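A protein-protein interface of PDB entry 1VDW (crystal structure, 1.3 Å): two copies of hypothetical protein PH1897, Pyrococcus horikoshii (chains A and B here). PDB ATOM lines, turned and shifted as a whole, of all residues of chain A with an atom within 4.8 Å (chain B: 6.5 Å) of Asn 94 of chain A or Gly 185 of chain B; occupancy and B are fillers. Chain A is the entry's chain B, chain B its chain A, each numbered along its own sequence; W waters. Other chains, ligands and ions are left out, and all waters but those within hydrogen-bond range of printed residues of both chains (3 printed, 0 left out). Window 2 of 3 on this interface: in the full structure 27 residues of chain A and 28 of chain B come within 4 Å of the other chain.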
ATOM      1  N   GLY A  26      18.571  14.536 -28.139  1.00  0.00           N
ATOM      2  CA  GLY A  26      17.633  15.051 -29.123  1.00  0.00           C
ATOM      3  C   GLY A  26      17.271  14.013 -30.168  1.00  0.00           C
ATOM      4  O   GLY A  26      16.878  14.352 -31.285  1.00  0.00           O
ATOM      5  N   TYR A  90      13.983  16.949 -19.965  1.00  0.00           N
ATOM      6  CA  TYR A  90      13.155  17.524 -21.022  1.00  0.00           C
ATOM      7  C   TYR A  90      14.065  18.141 -22.085  1.00  0.00           C
ATOM      8  O   TYR A  90      13.879  17.946 -23.286  1.00  0.00           O
ATOM      9  CB  TYR A  90      12.232  18.620 -20.479  1.00  0.00           C
ATOM     10  CG  TYR A  90      11.444  19.297 -21.581  1.00  0.00           C
ATOM     11  CD1 TYR A  90      10.234  18.763 -22.027  1.00  0.00           C
ATOM     12  CD2 TYR A  90      11.947  20.428 -22.235  1.00  0.00           C
ATOM     13  CE1 TYR A  90       9.546  19.334 -23.097  1.00  0.00           C
ATOM     14  CE2 TYR A  90      11.265  21.001 -23.307  1.00  0.00           C
ATOM     15  CZ  TYR A  90      10.068  20.447 -23.732  1.00  0.00           C
ATOM     16  OH  TYR A  90       9.398  20.991 -24.809  1.00  0.00           O
ATOM     17  N   ASN A  91      15.052  18.901 -21.626  1.00  0.00           N
ATOM     18  CA  ASN A  91      15.984  19.540 -22.543  1.00  0.00           C
ATOM     19  C   ASN A  91      16.680  18.498 -23.407  1.00  0.00           C
ATOM     20  O   ASN A  91      16.730  18.620 -24.629  1.00  0.00           O
ATOM     21  CB  ASN A  91      17.046  20.330 -21.779  1.00  0.00           C
ATOM     22  CG  ASN A  91      16.520  21.616 -21.177  1.00  0.00           C
ATOM     23  OD1 ASN A  91      15.405  22.070 -21.468  1.00  0.00           O
ATOM     24  ND2 ASN A  91      17.345  22.230 -20.339  1.00  0.00           N
ATOM     25  N   PHE A  92      17.211  17.464 -22.763  1.00  0.00           N
ATOM     26  CA  PHE A  92      17.929  16.415 -23.479  1.00  0.00           C
ATOM     27  C   PHE A  92      17.100  15.785 -24.587  1.00  0.00           C
ATOM     28  O   PHE A  92      17.540  15.700 -25.730  1.00  0.00           O
ATOM     29  CB  PHE A  92      18.379  15.325 -22.502  1.00  0.00           C
ATOM     30  CG  PHE A  92      19.201  14.236 -23.137  1.00  0.00           C
ATOM     31  CD1 PHE A  92      20.586  14.348 -23.228  1.00  0.00           C
ATOM     32  CD2 PHE A  92      18.588  13.094 -23.639  1.00  0.00           C
ATOM     33  CE1 PHE A  92      21.351  13.335 -23.808  1.00  0.00           C
ATOM     34  CE2 PHE A  92      19.342  12.075 -24.223  1.00  0.00           C
ATOM     35  CZ  PHE A  92      20.726  12.196 -24.307  1.00  0.00           C
ATOM     36  N   ILE A  93      15.890  15.370 -24.231  1.00  0.00           N
ATOM     37  CA  ILE A  93      14.967  14.735 -25.163  1.00  0.00           C
ATOM     38  C   ILE A  93      14.594  15.652 -26.328  1.00  0.00           C
ATOM     39  O   ILE A  93      14.297  15.189 -27.428  1.00  0.00           O
ATOM     40  CB  ILE A  93      13.674  14.309 -24.427  1.00  0.00           C
ATOM     41  CG1 ILE A  93      14.011  13.279 -23.344  1.00  0.00           C
ATOM     42  CG2 ILE A  93      12.662  13.751 -25.418  1.00  0.00           C
ATOM     43  CD1 ILE A  93      12.827  12.859 -22.500  1.00  0.00           C
ATOM     44  N   ASN A  94      14.626  16.956 -26.080  1.00  0.00           N
ATOM     45  CA  ASN A  94      14.269  17.943 -27.092  1.00  0.00           C
ATOM     46  C   ASN A  94      15.457  18.630 -27.754  1.00  0.00           C
ATOM     47  O   ASN A  94      15.285  19.642 -28.439  1.00  0.00           O
ATOM     48  CB  ASN A  94      13.319  18.976 -26.489  1.00  0.00           C
ATOM     49  CG  ASN A  94      11.920  18.431 -26.326  1.00  0.00           C
ATOM     50  OD1 ASN A  94      11.134  18.423 -27.280  1.00  0.00           O
ATOM     51  ND2 ASN A  94      11.605  17.947 -25.130  1.00  0.00           N
ATOM     52  N   GLY A  95      16.652  18.082 -27.555  1.00  0.00           N
ATOM     53  CA  GLY A  95      17.839  18.649 -28.175  1.00  0.00           C
ATOM     54  C   GLY A  95      18.289  20.012 -27.682  1.00  0.00           C
ATOM     55  O   GLY A  95      18.998  20.723 -28.397  1.00  0.00           O
ATOM     56  N   ILE A  96      17.884  20.384 -26.475  1.00  0.00           N
ATOM     57  CA  ILE A  96      18.277  21.662 -25.885  1.00  0.00           C
ATOM     58  C   ILE A  96      19.537  21.316 -25.098  1.00  0.00           C
ATOM     59  O   ILE A  96      19.486  20.529 -24.154  1.00  0.00           O
ATOM     60  CB  ILE A  96      17.151  22.189 -24.986  1.00  0.00           C
ATOM     61  CG1 ILE A  96      15.910  22.452 -25.847  1.00  0.00           C
ATOM     62  CG2 ILE A  96      17.595  23.464 -24.272  1.00  0.00           C
ATOM     63  CD1 ILE A  96      14.706  22.908 -25.074  1.00  0.00           C
ATOM     64  N   ARG B 123      24.409  23.282 -35.483  1.00  0.00           N
ATOM     65  CA  ARG B 123      23.119  23.291 -36.157  1.00  0.00           C
ATOM     66  C   ARG B 123      22.862  24.498 -37.030  1.00  0.00           C
ATOM     67  O   ARG B 123      23.032  25.640 -36.594  1.00  0.00           O
ATOM     68  CB  ARG B 123      21.986  23.229 -35.141  1.00  0.00           C
ATOM     69  CG  ARG B 123      21.807  21.924 -34.447  1.00  0.00           C
ATOM     70  CD  ARG B 123      20.731  22.127 -33.404  1.00  0.00           C
ATOM     71  NE  ARG B 123      20.558  20.974 -32.542  1.00  0.00           N
ATOM     72  CZ  ARG B 123      19.931  21.005 -31.370  1.00  0.00           C
ATOM     73  NH1 ARG B 123      19.408  22.142 -30.901  1.00  0.00           N
ATOM     74  NH2 ARG B 123      19.831  19.890 -30.662  1.00  0.00           N
ATOM     75  N   ILE B 140      11.832  20.681 -40.975  1.00  0.00           N
ATOM     76  CA  ILE B 140      11.336  20.785 -39.608  1.00  0.00           C
ATOM     77  C   ILE B 140       9.980  21.473 -39.612  1.00  0.00           C
ATOM     78  O   ILE B 140       9.648  22.212 -40.538  1.00  0.00           O
ATOM     79  CB  ILE B 140      12.298  21.595 -38.684  1.00  0.00           C
ATOM     80  CG1 ILE B 140      12.577  22.981 -39.274  1.00  0.00           C
ATOM     81  CG2 ILE B 140      13.580  20.803 -38.455  1.00  0.00           C
ATOM     82  CD1 ILE B 140      13.334  23.913 -38.329  1.00  0.00           C
ATOM     83  N   LYS B 141       9.191  21.216 -38.578  1.00  0.00           N
ATOM     84  CA  LYS B 141       7.878  21.834 -38.446  1.00  0.00           C
ATOM     85  C   LYS B 141       7.528  21.928 -36.973  1.00  0.00           C
ATOM     86  O   LYS B 141       8.082  21.197 -36.149  1.00  0.00           O
ATOM     87  CB  LYS B 141       6.807  21.016 -39.181  1.00  0.00           C
ATOM     88  CG  LYS B 141       6.631  19.596 -38.672  1.00  0.00           C
ATOM     89  CD  LYS B 141       5.636  18.833 -39.540  1.00  0.00           C
ATOM     90  CE  LYS B 141       5.511  17.375 -39.118  1.00  0.00           C
ATOM     91  NZ  LYS B 141       4.905  17.219 -37.767  1.00  0.00           N
ATOM     92  N   VAL B 142       6.622  22.837 -36.633  1.00  0.00           N
ATOM     93  CA  VAL B 142       6.214  22.969 -35.243  1.00  0.00           C
ATOM     94  C   VAL B 142       5.536  21.666 -34.848  1.00  0.00           C
ATOM     95  O   VAL B 142       5.012  20.940 -35.702  1.00  0.00           O
ATOM     96  CB  VAL B 142       5.226  24.146 -35.032  1.00  0.00           C
ATOM     97  CG1 VAL B 142       5.913  25.458 -35.351  1.00  0.00           C
ATOM     98  CG2 VAL B 142       3.976  23.967 -35.900  1.00  0.00           C
ATOM     99  N   ARG B 143       5.571  21.345 -33.564  1.00  0.00           N
ATOM    100  CA  ARG B 143       4.929  20.122 -33.114  1.00  0.00           C
ATOM    101  C   ARG B 143       3.460  20.389 -32.830  1.00  0.00           C
ATOM    102  O   ARG B 143       3.036  21.532 -32.671  1.00  0.00           O
ATOM    103  CB  ARG B 143       5.608  19.584 -31.853  1.00  0.00           C
ATOM    104  CG  ARG B 143       5.416  20.432 -30.601  1.00  0.00           C
ATOM    105  CD  ARG B 143       6.176  19.807 -29.440  1.00  0.00           C
ATOM    106  NE  ARG B 143       6.089  20.576 -28.204  1.00  0.00           N
ATOM    107  CZ  ARG B 143       6.974  20.487 -27.216  1.00  0.00           C
ATOM    108  NH1 ARG B 143       8.016  19.672 -27.325  1.00  0.00           N
ATOM    109  NH2 ARG B 143       6.811  21.194 -26.110  1.00  0.00           N
ATOM    110  N   ALA B 180      13.864  29.257 -32.987  1.00  0.00           N
ATOM    111  CA  ALA B 180      14.285  28.103 -33.776  1.00  0.00           C
ATOM    112  C   ALA B 180      13.780  26.823 -33.105  1.00  0.00           C
ATOM    113  O   ALA B 180      13.387  25.868 -33.781  1.00  0.00           O
ATOM    114  CB  ALA B 180      15.808  28.071 -33.895  1.00  0.00           C
ATOM    115  N   TYR B 181      13.805  26.799 -31.775  1.00  0.00           N
ATOM    116  CA  TYR B 181      13.335  25.634 -31.035  1.00  0.00           C
ATOM    117  C   TYR B 181      11.841  25.456 -31.270  1.00  0.00           C
ATOM    118  O   TYR B 181      11.361  24.332 -31.415  1.00  0.00           O
ATOM    119  CB  TYR B 181      13.618  25.785 -29.540  1.00  0.00           C
ATOM    120  CG  TYR B 181      15.080  25.665 -29.148  1.00  0.00           C
ATOM    121  CD1 TYR B 181      16.069  25.338 -30.081  1.00  0.00           C
ATOM    122  CD2 TYR B 181      15.472  25.893 -27.831  1.00  0.00           C
ATOM    123  CE1 TYR B 181      17.417  25.248 -29.704  1.00  0.00           C
ATOM    124  CE2 TYR B 181      16.805  25.806 -27.449  1.00  0.00           C
ATOM    125  CZ  TYR B 181      17.768  25.485 -28.387  1.00  0.00           C
ATOM    126  OH  TYR B 181      19.082  25.423 -27.983  1.00  0.00           O
ATOM    127  N   LEU B 182      11.106  26.564 -31.293  1.00  0.00           N
ATOM    128  CA  LEU B 182       9.676  26.506 -31.571  1.00  0.00           C
ATOM    129  C   LEU B 182       9.480  25.926 -32.976  1.00  0.00           C
ATOM    130  O   LEU B 182       8.628  25.060 -33.196  1.00  0.00           O
ATOM    131  CB  LEU B 182       9.079  27.912 -31.511  1.00  0.00           C
ATOM    132  CG  LEU B 182       7.659  28.093 -32.051  1.00  0.00           C
ATOM    133  CD1 LEU B 182       6.668  27.307 -31.207  1.00  0.00           C
ATOM    134  CD2 LEU B 182       7.317  29.574 -32.054  1.00  0.00           C
ATOM    135  N   ALA B 183      10.299  26.392 -33.914  1.00  0.00           N
ATOM    136  CA  ALA B 183      10.212  25.960 -35.300  1.00  0.00           C
ATOM    137  C   ALA B 183      10.402  24.465 -35.510  1.00  0.00           C
ATOM    138  O   ALA B 183       9.809  23.888 -36.423  1.00  0.00           O
ATOM    139  CB  ALA B 183      11.216  26.731 -36.145  1.00  0.00           C
ATOM    140  N   ARG B 184      11.226  23.825 -34.686  1.00  0.00           N
ATOM    141  CA  ARG B 184      11.448  22.394 -34.872  1.00  0.00           C
ATOM    142  C   ARG B 184      10.695  21.511 -33.886  1.00  0.00           C
ATOM    143  O   ARG B 184      10.869  20.293 -33.879  1.00  0.00           O
ATOM    144  CB  ARG B 184      12.945  22.063 -34.850  1.00  0.00           C
ATOM    145  CG  ARG B 184      13.642  22.271 -33.523  1.00  0.00           C
ATOM    146  CD  ARG B 184      15.091  21.791 -33.597  1.00  0.00           C
ATOM    147  NE  ARG B 184      15.817  22.060 -32.359  1.00  0.00           N
ATOM    148  CZ  ARG B 184      15.684  21.354 -31.241  1.00  0.00           C
ATOM    149  NH1 ARG B 184      14.861  20.317 -31.198  1.00  0.00           N
ATOM    150  NH2 ARG B 184      16.346  21.711 -30.151  1.00  0.00           N
ATOM    151  N   GLY B 185       9.872  22.122 -33.043  1.00  0.00           N
ATOM    152  CA  GLY B 185       9.074  21.349 -32.105  1.00  0.00           C
ATOM    153  C   GLY B 185       9.625  21.052 -30.722  1.00  0.00           C
ATOM    154  O   GLY B 185       9.202  20.082 -30.090  1.00  0.00           O
ATOM    155  N   ALA B 186      10.550  21.878 -30.241  1.00  0.00           N
ATOM    156  CA  ALA B 186      11.135  21.691 -28.916  1.00  0.00           C
ATOM    157  C   ALA B 186      10.411  22.536 -27.866  1.00  0.00           C
ATOM    158  O   ALA B 186      10.627  22.363 -26.667  1.00  0.00           O
ATOM    159  CB  ALA B 186      12.615  22.043 -28.952  1.00  0.00           C
ATOM    160  N   LEU B 187       9.563  23.450 -28.336  1.00  0.00           N
ATOM    161  CA  LEU B 187       8.758  24.331 -27.489  1.00  0.00           C
ATOM    162  C   LEU B 187       7.422  24.540 -28.192  1.00  0.00           C
ATOM    163  O   LEU B 187       7.325  24.374 -29.411  1.00  0.00           O
ATOM    164  CB  LEU B 187       9.429  25.698 -27.305  1.00  0.00           C
ATOM    165  CG  LEU B 187      10.717  25.765 -26.485  1.00  0.00           C
ATOM    166  CD1 LEU B 187      11.296  27.176 -26.581  1.00  0.00           C
ATOM    167  CD2 LEU B 187      10.440  25.380 -25.040  1.00  0.00           C
ATOM    168  N   ASP B 188       6.398  24.911 -27.426  1.00  0.00           N
ATOM    169  CA  ASP B 188       5.072  25.161 -27.988  1.00  0.00           C
ATOM    170  C   ASP B 188       4.840  26.647 -28.237  1.00  0.00           C
ATOM    171  O   ASP B 188       4.011  27.019 -29.065  1.00  0.00           O
ATOM    172  CB  ASP B 188       3.994  24.629 -27.049  1.00  0.00           C
ATOM    173  CG  ASP B 188       4.116  23.141 -26.818  1.00  0.00           C
ATOM    174  OD1 ASP B 188       3.822  22.363 -27.751  1.00  0.00           O
ATOM    175  OD2 ASP B 188       4.520  22.757 -25.703  1.00  0.00           O
HETATM  176  O   HOH W   1      12.391  18.449 -29.999  1.00  0.00           O
HETATM  177  O   HOH W   2       9.318  16.618 -28.320  1.00  0.00           O
HETATM  178  O   HOH W   3      16.948  17.728 -31.608  1.00  0.00           O
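NH2 of Arg 184 of chain B lies within hydrogen-bond range of O of Gly 95 of chain A.
The guanidinium group (NH1) of Arg 184 of chain B lies within hydrogen-bond range of the backbone carbonyl oxygen (O) of Asn 94 of chain A (2.9 Å).
NH1 of Arg 143 of chain B sits at hydrogen-bond distance from OD1 of Asn 94 of chain A.
The guanidinium group of Arg 123 of chain B is in hydrogen-bond range of the backbone carbonyl oxygen of Gly 95 of chain A, at 2.6 Å.
The side-chain hydroxyl (OH) of Tyr 90 of chain A is in hydrogen-bond range of the backbone carbonyl oxygen (O) of Ala 186 of chain B.
The side-chain hydroxyl of Tyr 90 of chain A is in hydrogen-bond range of the guanidinium group of Arg 143 of chain B (2.9 Å).
The backbone NH (N) of Ala 186 of chain B lies within hydrogen-bond range of the backbone carbonyl oxygen (O) of Tyr 181 of chain B, 2.8 Å away.
The backbone carbonyl oxygen of Gly 185 of chain B lies within hydrogen-bond range of the guanidinium group of Arg 143 of chain B.
O of Asn 91 of chain A lies within hydrogen-bond range of N of Ile 96 of chain A (2.8 Å).
The guanidinium group (NH2) of Arg 143 of chain B is in salt-bridge range of the side-chain carboxylate (OD2) of Asp 188 of chain B (2.8 Å).
The side-chain amide nitrogen (ND2) of Asn 94 of chain A sits at hydrogen-bond distance from the backbone carbonyl oxygen (O) of Tyr 90 of chain A (2.9 Å).
Asn 94 of chain A touches Gly 185 of chain B.
Asn 94 of chain A touches Ala 186 of chain B.
Tyr 181 of chain B touches Ile 96 of chain A.
Asn 94 of chain A touches just these residues of chain B: Arg 143 (3.4 Å), Arg 184 (2.9 Å), Gly 185 (3.8 Å) and Ala 186 (3.6 Å).
Of the printed residues of chain B, Gly 95 of chain A touches Arg 123 (2.6 Å) and Arg 184 (3.3 Å).
Lys 141 of chain B touches none of the printed residues of chain A.
Printed residues of chain A within 4 Å of Arg 143 of chain B: Tyr 90 and Asn 94.
Printed residues of chain A within 4 Å of Arg 184 of chain B: Asn 94 (2.9 Å) and Gly 95 (3.3 Å).
Gly 185 of chain B touches just one residue of chain A: Asn 94 (3.8 Å).
The nearest printed residue of chain A that does not touch Arg 184 of chain B is Ile 96 of chain A (4.2 Å).
Hydrophobic or aromatic side chains of chain A within 4 Å of the printed part of chain B: Tyr 90 and Ile 96.
Along chain A the printed residues that touch a printed residue of chain B span positions 90 to 96.
Hydrophobic or aromatic side chains of chain B that line the printed part of chain A: Tyr 181 and Ala 186.
Among the printed residues, no Asp or Glu carboxylate lies within 4 Å of a Lys or Arg side-chain nitrogen of the other chain.
No position is printed for both chains.
Water W2 bridges the side-chain amide oxygen (OD1) of Asn 94 of chain A and the guanidinium group (NH1) of Arg 143 of chain B.
Water W1 lies within hydrogen-bond range of the side-chain amide oxygen of Asn 94 of chain A (3.0 Å) and the guanidinium group of Arg 184 of chain B (3.3 Å).
Water W3 bridges the guanidinium group of Arg 184 of chain B (3.4 Å) and the backbone carbonyl oxygen of Gly 26 of chain A (3.4 Å).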
